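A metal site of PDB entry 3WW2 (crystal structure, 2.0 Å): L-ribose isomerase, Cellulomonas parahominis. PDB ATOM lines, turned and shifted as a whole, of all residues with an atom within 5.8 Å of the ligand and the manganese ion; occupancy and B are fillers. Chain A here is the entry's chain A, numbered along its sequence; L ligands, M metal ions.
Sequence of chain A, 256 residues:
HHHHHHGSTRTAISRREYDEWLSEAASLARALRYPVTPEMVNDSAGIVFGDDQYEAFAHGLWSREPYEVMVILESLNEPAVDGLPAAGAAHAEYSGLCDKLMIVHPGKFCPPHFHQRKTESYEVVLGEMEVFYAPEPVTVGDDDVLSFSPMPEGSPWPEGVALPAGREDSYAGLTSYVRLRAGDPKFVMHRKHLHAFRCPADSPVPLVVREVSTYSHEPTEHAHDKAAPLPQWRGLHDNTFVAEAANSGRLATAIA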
ATOM      1  N   ILE A  47       1.345 -20.881 -12.690  1.00  0.00           N
ATOM      2  CA  ILE A  47       0.975 -19.816 -13.628  1.00  0.00           C
ATOM      3  C   ILE A  47       2.127 -19.138 -14.394  1.00  0.00           C
ATOM      4  O   ILE A  47       3.124 -18.734 -13.817  1.00  0.00           O
ATOM      5  CB  ILE A  47       0.175 -18.702 -12.880  1.00  0.00           C
ATOM      6  CG1 ILE A  47      -0.949 -19.349 -12.074  1.00  0.00           C
ATOM      7  CG2 ILE A  47      -0.378 -17.685 -13.858  1.00  0.00           C
ATOM      8  CD1 ILE A  47      -1.777 -18.359 -11.277  1.00  0.00           C
ATOM      9  N   PHE A  49       2.480 -15.955 -16.764  1.00  0.00           N
ATOM     10  CA  PHE A  49       1.761 -14.767 -17.256  1.00  0.00           C
ATOM     11  C   PHE A  49       2.154 -14.266 -18.648  1.00  0.00           C
ATOM     12  O   PHE A  49       2.833 -13.253 -18.773  1.00  0.00           O
ATOM     13  CB  PHE A  49       1.929 -13.615 -16.255  1.00  0.00           C
ATOM     14  CG  PHE A  49       1.268 -13.875 -14.924  1.00  0.00           C
ATOM     15  CD1 PHE A  49      -0.099 -13.700 -14.766  1.00  0.00           C
ATOM     16  CD2 PHE A  49       2.022 -14.353 -13.854  1.00  0.00           C
ATOM     17  CE1 PHE A  49      -0.725 -14.008 -13.557  1.00  0.00           C
ATOM     18  CE2 PHE A  49       1.416 -14.662 -12.632  1.00  0.00           C
ATOM     19  CZ  PHE A  49       0.033 -14.488 -12.479  1.00  0.00           C
ATOM     20  N   MET A  70       4.674 -17.945 -11.315  1.00  0.00           N
ATOM     21  CA  MET A  70       4.433 -18.283  -9.910  1.00  0.00           C
ATOM     22  C   MET A  70       3.518 -19.487  -9.728  1.00  0.00           C
ATOM     23  O   MET A  70       2.820 -19.908 -10.653  1.00  0.00           O
ATOM     24  CB  MET A  70       3.814 -17.071  -9.186  1.00  0.00           C
ATOM     25  CG  MET A  70       2.291 -16.943  -9.363  1.00  0.00           C
ATOM     26  SD  MET A  70       1.627 -15.360  -8.734  1.00  0.00           S
ATOM     27  CE  MET A  70       1.702 -15.573  -6.983  1.00  0.00           C
ATOM     28  N   ILE A  72       0.436 -21.128  -7.253  1.00  0.00           N
ATOM     29  CA  ILE A  72      -0.552 -20.781  -6.270  1.00  0.00           C
ATOM     30  C   ILE A  72      -1.271 -22.048  -5.838  1.00  0.00           C
ATOM     31  O   ILE A  72      -1.701 -22.841  -6.666  1.00  0.00           O
ATOM     32  CB  ILE A  72      -1.557 -19.756  -6.832  1.00  0.00           C
ATOM     33  CG1 ILE A  72      -0.808 -18.471  -7.206  1.00  0.00           C
ATOM     34  CG2 ILE A  72      -2.632 -19.459  -5.805  1.00  0.00           C
ATOM     35  CD1 ILE A  72      -1.679 -17.402  -7.864  1.00  0.00           C
ATOM     36  N   LYS A 100      -4.924 -18.757   0.094  1.00  0.00           N
ATOM     37  CA  LYS A 100      -4.019 -19.419  -0.831  1.00  0.00           C
ATOM     38  C   LYS A 100      -2.575 -19.149  -0.478  1.00  0.00           C
ATOM     39  O   LYS A 100      -2.234 -18.101   0.093  1.00  0.00           O
ATOM     40  CB  LYS A 100      -4.309 -18.968  -2.270  1.00  0.00           C
ATOM     41  CG  LYS A 100      -4.453 -17.467  -2.428  1.00  0.00           C
ATOM     42  CD  LYS A 100      -4.723 -17.077  -3.877  1.00  0.00           C
ATOM     43  CE  LYS A 100      -5.947 -17.787  -4.460  1.00  0.00           C
ATOM     44  NZ  LYS A 100      -6.347 -17.182  -5.778  1.00  0.00           N
ATOM     45  N   MET A 102       1.212 -18.727  -1.959  1.00  0.00           N
ATOM     46  CA  MET A 102       1.905 -18.392  -3.198  1.00  0.00           C
ATOM     47  C   MET A 102       3.408 -18.591  -3.118  1.00  0.00           C
ATOM     48  O   MET A 102       4.043 -18.223  -2.125  1.00  0.00           O
ATOM     49  CB  MET A 102       1.574 -16.952  -3.583  1.00  0.00           C
ATOM     50  CG  MET A 102       0.067 -16.727  -3.700  1.00  0.00           C
ATOM     51  SD  MET A 102      -0.359 -15.062  -4.194  1.00  0.00           S
ATOM     52  CE  MET A 102      -0.241 -14.191  -2.626  1.00  0.00           C
ATOM     53  N   CYS A 110       4.849 -11.450  -9.678  1.00  0.00           N
ATOM     54  CA  CYS A 110       3.415 -11.651  -9.779  1.00  0.00           C
ATOM     55  C   CYS A 110       3.160 -10.250 -10.366  1.00  0.00           C
ATOM     56  O   CYS A 110       3.180  -9.268  -9.633  1.00  0.00           O
ATOM     57  CB  CYS A 110       2.750 -11.765  -8.412  1.00  0.00           C
ATOM     58  SG  CYS A 110       0.953 -11.546  -8.529  1.00  0.00           S
ATOM     59  N   HIS A 113      -1.442  -5.633 -11.639  1.00  0.00           N
ATOM     60  CA  HIS A 113      -2.877  -5.836 -11.861  1.00  0.00           C
ATOM     61  C   HIS A 113      -3.665  -5.246 -10.701  1.00  0.00           C
ATOM     62  O   HIS A 113      -3.097  -4.717  -9.734  1.00  0.00           O
ATOM     63  CB  HIS A 113      -3.205  -7.325 -11.969  1.00  0.00           C
ATOM     64  CG  HIS A 113      -3.023  -8.076 -10.689  1.00  0.00           C
ATOM     65  ND1 HIS A 113      -1.791  -8.548 -10.272  1.00  0.00           N
ATOM     66  CD2 HIS A 113      -3.890  -8.363  -9.690  1.00  0.00           C
ATOM     67  CE1 HIS A 113      -1.913  -9.083  -9.067  1.00  0.00           C
ATOM     68  NE2 HIS A 113      -3.183  -8.979  -8.689  1.00  0.00           N
ATOM     69  N   HIS A 115      -7.904  -5.682  -8.776  1.00  0.00           N
ATOM     70  CA  HIS A 115      -9.130  -6.452  -8.726  1.00  0.00           C
ATOM     71  C   HIS A 115     -10.267  -5.463  -8.534  1.00  0.00           C
ATOM     72  O   HIS A 115     -10.088  -4.429  -7.883  1.00  0.00           O
ATOM     73  CB  HIS A 115      -9.091  -7.434  -7.554  1.00  0.00           C
ATOM     74  CG  HIS A 115      -7.907  -8.345  -7.581  1.00  0.00           C
ATOM     75  ND1 HIS A 115      -7.693  -9.266  -8.587  1.00  0.00           N
ATOM     76  CD2 HIS A 115      -6.848  -8.463  -6.743  1.00  0.00           C
ATOM     77  CE1 HIS A 115      -6.551  -9.897  -8.369  1.00  0.00           C
ATOM     78  NE2 HIS A 115      -6.018  -9.427  -7.249  1.00  0.00           N
ATOM     79  N   LYS A 118     -11.981  -8.145  -5.310  1.00  0.00           N
ATOM     80  CA  LYS A 118     -11.103  -8.715  -4.288  1.00  0.00           C
ATOM     81  C   LYS A 118     -10.167  -7.783  -3.511  1.00  0.00           C
ATOM     82  O   LYS A 118      -9.410  -7.017  -4.073  1.00  0.00           O
ATOM     83  CB  LYS A 118     -10.283  -9.852  -4.896  1.00  0.00           C
ATOM     84  CG  LYS A 118      -9.578 -10.727  -3.878  1.00  0.00           C
ATOM     85  CD  LYS A 118      -8.795 -11.853  -4.546  1.00  0.00           C
ATOM     86  CE  LYS A 118      -7.569 -11.329  -5.255  1.00  0.00           C
ATOM     87  NZ  LYS A 118      -6.713 -12.428  -5.791  1.00  0.00           N
ATOM     88  N   GLU A 120      -7.238  -8.023  -0.623  1.00  0.00           N
ATOM     89  CA  GLU A 120      -6.344  -9.050  -0.096  1.00  0.00           C
ATOM     90  C   GLU A 120      -5.380  -8.606   1.007  1.00  0.00           C
ATOM     91  O   GLU A 120      -5.201  -7.412   1.268  1.00  0.00           O
ATOM     92  CB  GLU A 120      -5.553  -9.678  -1.254  1.00  0.00           C
ATOM     93  CG  GLU A 120      -5.190  -8.702  -2.373  1.00  0.00           C
ATOM     94  CD  GLU A 120      -4.465  -9.383  -3.540  1.00  0.00           C
ATOM     95  OE1 GLU A 120      -3.250  -9.659  -3.422  1.00  0.00           O
ATOM     96  OE2 GLU A 120      -5.115  -9.647  -4.568  1.00  0.00           O
ATOM     97  N   TYR A 122      -1.499  -9.941   2.994  1.00  0.00           N
ATOM     98  CA  TYR A 122      -0.316 -10.770   2.844  1.00  0.00           C
ATOM     99  C   TYR A 122       0.373 -11.132   4.140  1.00  0.00           C
ATOM    100  O   TYR A 122       0.503 -10.312   5.057  1.00  0.00           O
ATOM    101  CB  TYR A 122       0.718 -10.089   1.949  1.00  0.00           C
ATOM    102  CG  TYR A 122       0.159  -9.548   0.655  1.00  0.00           C
ATOM    103  CD1 TYR A 122      -0.544 -10.381  -0.220  1.00  0.00           C
ATOM    104  CD2 TYR A 122       0.356  -8.219   0.295  1.00  0.00           C
ATOM    105  CE1 TYR A 122      -1.044  -9.889  -1.416  1.00  0.00           C
ATOM    106  CE2 TYR A 122      -0.125  -7.715  -0.905  1.00  0.00           C
ATOM    107  CZ  TYR A 122      -0.821  -8.552  -1.763  1.00  0.00           C
ATOM    108  OH  TYR A 122      -1.299  -8.050  -2.954  1.00  0.00           O
ATOM    109  N   HIS A 195      -1.157  -3.347  -8.112  1.00  0.00           N
ATOM    110  CA  HIS A 195      -0.101  -3.939  -7.294  1.00  0.00           C
ATOM    111  C   HIS A 195       0.637  -5.072  -8.012  1.00  0.00           C
ATOM    112  O   HIS A 195       0.169  -5.629  -9.002  1.00  0.00           O
ATOM    113  CB  HIS A 195      -0.650  -4.448  -5.965  1.00  0.00           C
ATOM    114  CG  HIS A 195      -1.650  -5.555  -6.111  1.00  0.00           C
ATOM    115  ND1 HIS A 195      -2.956  -5.344  -6.472  1.00  0.00           N
ATOM    116  CD2 HIS A 195      -1.516  -6.897  -5.945  1.00  0.00           C
ATOM    117  CE1 HIS A 195      -3.593  -6.504  -6.529  1.00  0.00           C
ATOM    118  NE2 HIS A 195      -2.738  -7.461  -6.210  1.00  0.00           N
ATOM    119  N   PHE A 197       4.371  -7.858  -7.091  1.00  0.00           N
ATOM    120  CA  PHE A 197       5.394  -8.154  -6.105  1.00  0.00           C
ATOM    121  C   PHE A 197       6.391  -9.188  -6.604  1.00  0.00           C
ATOM    122  O   PHE A 197       6.102  -9.965  -7.504  1.00  0.00           O
ATOM    123  CB  PHE A 197       4.737  -8.594  -4.795  1.00  0.00           C
ATOM    124  CG  PHE A 197       4.036  -9.916  -4.875  1.00  0.00           C
ATOM    125  CD1 PHE A 197       4.731 -11.116  -4.683  1.00  0.00           C
ATOM    126  CD2 PHE A 197       2.660  -9.977  -5.086  1.00  0.00           C
ATOM    127  CE1 PHE A 197       4.076 -12.347  -4.716  1.00  0.00           C
ATOM    128  CE2 PHE A 197       1.996 -11.203  -5.115  1.00  0.00           C
ATOM    129  CZ  PHE A 197       2.702 -12.387  -4.923  1.00  0.00           C
ATOM    130  N   GLU A 211      -1.889 -15.720   1.211  1.00  0.00           N
ATOM    131  CA  GLU A 211      -2.832 -14.672   0.860  1.00  0.00           C
ATOM    132  C   GLU A 211      -4.198 -14.990   1.473  1.00  0.00           C
ATOM    133  O   GLU A 211      -4.737 -16.083   1.296  1.00  0.00           O
ATOM    134  CB  GLU A 211      -2.992 -14.555  -0.662  1.00  0.00           C
ATOM    135  CG  GLU A 211      -4.047 -13.532  -1.096  1.00  0.00           C
ATOM    136  CD  GLU A 211      -4.252 -13.469  -2.614  1.00  0.00           C
ATOM    137  OE1 GLU A 211      -3.280 -13.162  -3.341  1.00  0.00           O
ATOM    138  OE2 GLU A 211      -5.382 -13.739  -3.065  1.00  0.00           O
ATOM    139  N   SER A 216     -12.266 -15.228  -4.697  1.00  0.00           N
ATOM    140  CA  SER A 216     -11.432 -15.124  -5.879  1.00  0.00           C
ATOM    141  C   SER A 216     -12.155 -15.605  -7.148  1.00  0.00           C
ATOM    142  O   SER A 216     -12.295 -16.800  -7.381  1.00  0.00           O
ATOM    143  CB  SER A 216     -10.158 -15.946  -5.646  1.00  0.00           C
ATOM    144  OG  SER A 216      -9.285 -15.866  -6.750  1.00  0.00           O
ATOM    145  N   GLU A 218     -11.959 -16.477 -10.577  1.00  0.00           N
ATOM    146  CA  GLU A 218     -10.970 -16.826 -11.605  1.00  0.00           C
ATOM    147  C   GLU A 218     -11.447 -18.039 -12.403  1.00  0.00           C
ATOM    148  O   GLU A 218     -11.148 -19.174 -12.056  1.00  0.00           O
ATOM    149  CB  GLU A 218      -9.622 -17.155 -10.948  1.00  0.00           C
ATOM    150  CG  GLU A 218      -9.043 -16.030 -10.121  1.00  0.00           C
ATOM    151  CD  GLU A 218      -7.768 -16.419  -9.406  1.00  0.00           C
ATOM    152  OE1 GLU A 218      -7.797 -17.399  -8.613  1.00  0.00           O
ATOM    153  OE2 GLU A 218      -6.729 -15.757  -9.629  1.00  0.00           O
ATOM    154  N   ASN A 239      -9.665 -10.218 -12.323  1.00  0.00           N
ATOM    155  CA  ASN A 239      -8.255  -9.838 -12.435  1.00  0.00           C
ATOM    156  C   ASN A 239      -7.993  -9.050 -13.711  1.00  0.00           C
ATOM    157  O   ASN A 239      -8.218  -9.550 -14.803  1.00  0.00           O
ATOM    158  CB  ASN A 239      -7.338 -11.064 -12.433  1.00  0.00           C
ATOM    159  CG  ASN A 239      -7.580 -11.997 -11.263  1.00  0.00           C
ATOM    160  OD1 ASN A 239      -7.937 -11.552 -10.170  1.00  0.00           O
ATOM    161  ND2 ASN A 239      -7.375 -13.293 -11.486  1.00  0.00           N
ATOM    162  N   PHE A 241      -4.964  -7.261 -15.705  1.00  0.00           N
ATOM    163  CA  PHE A 241      -3.535  -7.048 -15.776  1.00  0.00           C
ATOM    164  C   PHE A 241      -3.202  -5.848 -16.634  1.00  0.00           C
ATOM    165  O   PHE A 241      -3.885  -5.568 -17.622  1.00  0.00           O
ATOM    166  CB  PHE A 241      -2.836  -8.296 -16.330  1.00  0.00           C
ATOM    167  CG  PHE A 241      -2.955  -9.501 -15.456  1.00  0.00           C
ATOM    168  CD1 PHE A 241      -4.015 -10.393 -15.607  1.00  0.00           C
ATOM    169  CD2 PHE A 241      -2.037  -9.717 -14.422  1.00  0.00           C
ATOM    170  CE1 PHE A 241      -4.162 -11.486 -14.751  1.00  0.00           C
ATOM    171  CE2 PHE A 241      -2.181 -10.812 -13.557  1.00  0.00           C
ATOM    172  CZ  PHE A 241      -3.242 -11.691 -13.726  1.00  0.00           C
ATOM    173  N   ARG A 250      -2.760 -15.987 -18.152  1.00  0.00           N
ATOM    174  CA  ARG A 250      -3.136 -16.357 -16.790  1.00  0.00           C
ATOM    175  C   ARG A 250      -4.274 -17.386 -16.724  1.00  0.00           C
ATOM    176  O   ARG A 250      -4.519 -17.974 -15.660  1.00  0.00           O
ATOM    177  CB  ARG A 250      -3.530 -15.086 -16.008  1.00  0.00           C
ATOM    178  CG  ARG A 250      -3.510 -15.220 -14.480  1.00  0.00           C
ATOM    179  CD  ARG A 250      -4.744 -15.920 -13.918  1.00  0.00           C
ATOM    180  NE  ARG A 250      -4.517 -16.402 -12.561  1.00  0.00           N
ATOM    181  CZ  ARG A 250      -5.371 -17.152 -11.881  1.00  0.00           C
ATOM    182  NH1 ARG A 250      -5.083 -17.557 -10.650  1.00  0.00           N
ATOM    183  NH2 ARG A 250      -6.524 -17.516 -12.433  1.00  0.00           N
HETATM  184  C1  LIG L   1      -1.818 -11.941  -6.345  1.00  0.00           C
HETATM  185  O1  LIG L   1      -1.963 -10.654  -5.753  1.00  0.00           O
HETATM  186  C2  LIG L   1      -3.139 -12.458  -6.879  1.00  0.00           C
HETATM  187  O2  LIG L   1      -4.208 -11.767  -6.246  1.00  0.00           O
HETATM  188  C3  LIG L   1      -3.322 -13.965  -6.740  1.00  0.00           C
HETATM  189  O3  LIG L   1      -4.177 -14.258  -5.638  1.00  0.00           O
HETATM  190  C4  LIG L   1      -4.002 -14.391  -8.046  1.00  0.00           C
HETATM  191  O4  LIG L   1      -5.395 -14.543  -7.833  1.00  0.00           O
HETATM  192  C5  LIG L   1      -3.764 -13.239  -9.021  1.00  0.00           C
HETATM  193  O5  LIG L   1      -3.188 -12.150  -8.279  1.00  0.00           O
HETATM  194  C6  LIG L   1      -2.802 -13.596 -10.139  1.00  0.00           C
HETATM  195  O6  LIG L   1      -3.516 -13.963 -11.308  1.00  0.00           O
HETATM  196 MN    MN M   1      -3.939  -9.499  -6.560  1.00  0.00          MN
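OE1 of Glu 211 lies within hydrogen-bond range of O3 of the ligand.
O3 of the ligand sits at hydrogen-bond distance from NZ of Lys 118 (3.1 Å).
The side-chain amino group (NZ) of Lys 100 sits at hydrogen-bond distance from an oxygen (O4) of the ligand (3.5 Å).
O6 of the ligand sits at hydrogen-bond distance from NE of Arg 250, at 2.9 Å.
The side-chain carboxylate (OE2) of Glu 218 lies within hydrogen-bond range of an oxygen (O4) of the ligand (2.5 Å).
NE2 of His 115 binds the manganese ion (2.2 Å).
O2 of the ligand is bound to the manganese ion, 2.3 Å away.
The manganese ion is bound by OE2 of Glu 120, 2.3 Å away.
NE2 of His 113 binds the manganese ion, 2.3 Å away.
A ring nitrogen (NE2) of His 195 binds the manganese ion.
The manganese ion is bound by O1 of the ligand, 2.4 Å away.
The manganese ion has six donor atoms within binding distance.
Merely in contact with the ligand: Phe 241 (3.3 Å), Cys 110 (3.6 Å), Phe 49 (3.6 Å), Ile 72 (3.8 Å), Tyr 122 (3.9 Å) and Asn 239 (3.9 Å).
Hydrophobic or aromatic side chains within 4 Å of the ligand: Phe 49, Ile 72, His 113, His 115, His 195 and Phe 241.
Of the 20 residues printed, 15 come within 4 Å of the ligand.
The nearest printed residue that does not touch the ligand is Phe 197 (4.05 Å).
Within 4 Å of the manganese ion: His 113, His 115, Glu 120 and His 195.
The nearest printed residue that does not touch the manganese ion is Lys 118 (4.1 Å).
The backbone NH (N) of Cys 110 sits at hydrogen-bond distance from the backbone carbonyl oxygen (O) of Phe 197 (2.9 Å).
O of Lys 100 is in hydrogen-bond range of N of Glu 211.
The side-chain hydroxyl (OH) of Tyr 122 sits at hydrogen-bond distance from the side-chain carboxylate (OE1) of Glu 120 (2.6 Å).
The side-chain carboxylate of Glu 218 is in hydrogen-bond range of the side-chain hydroxyl of Ser 216 (2.8 Å).
NZ of Lys 118 is in salt-bridge range of OE2 of Glu 211, 3.3 Å away.
The side-chain amino group (NZ) of Lys 118 lies close to a ring nitrogen (NE2) of His 115, at 3.4 Å.
ND1 of His 115 sits at hydrogen-bond distance from OD1 of Asn 239.
The guanidinium group (NH1) of Arg 250 lies within salt-bridge range of the side-chain carboxylate (OE2) of Glu 218.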
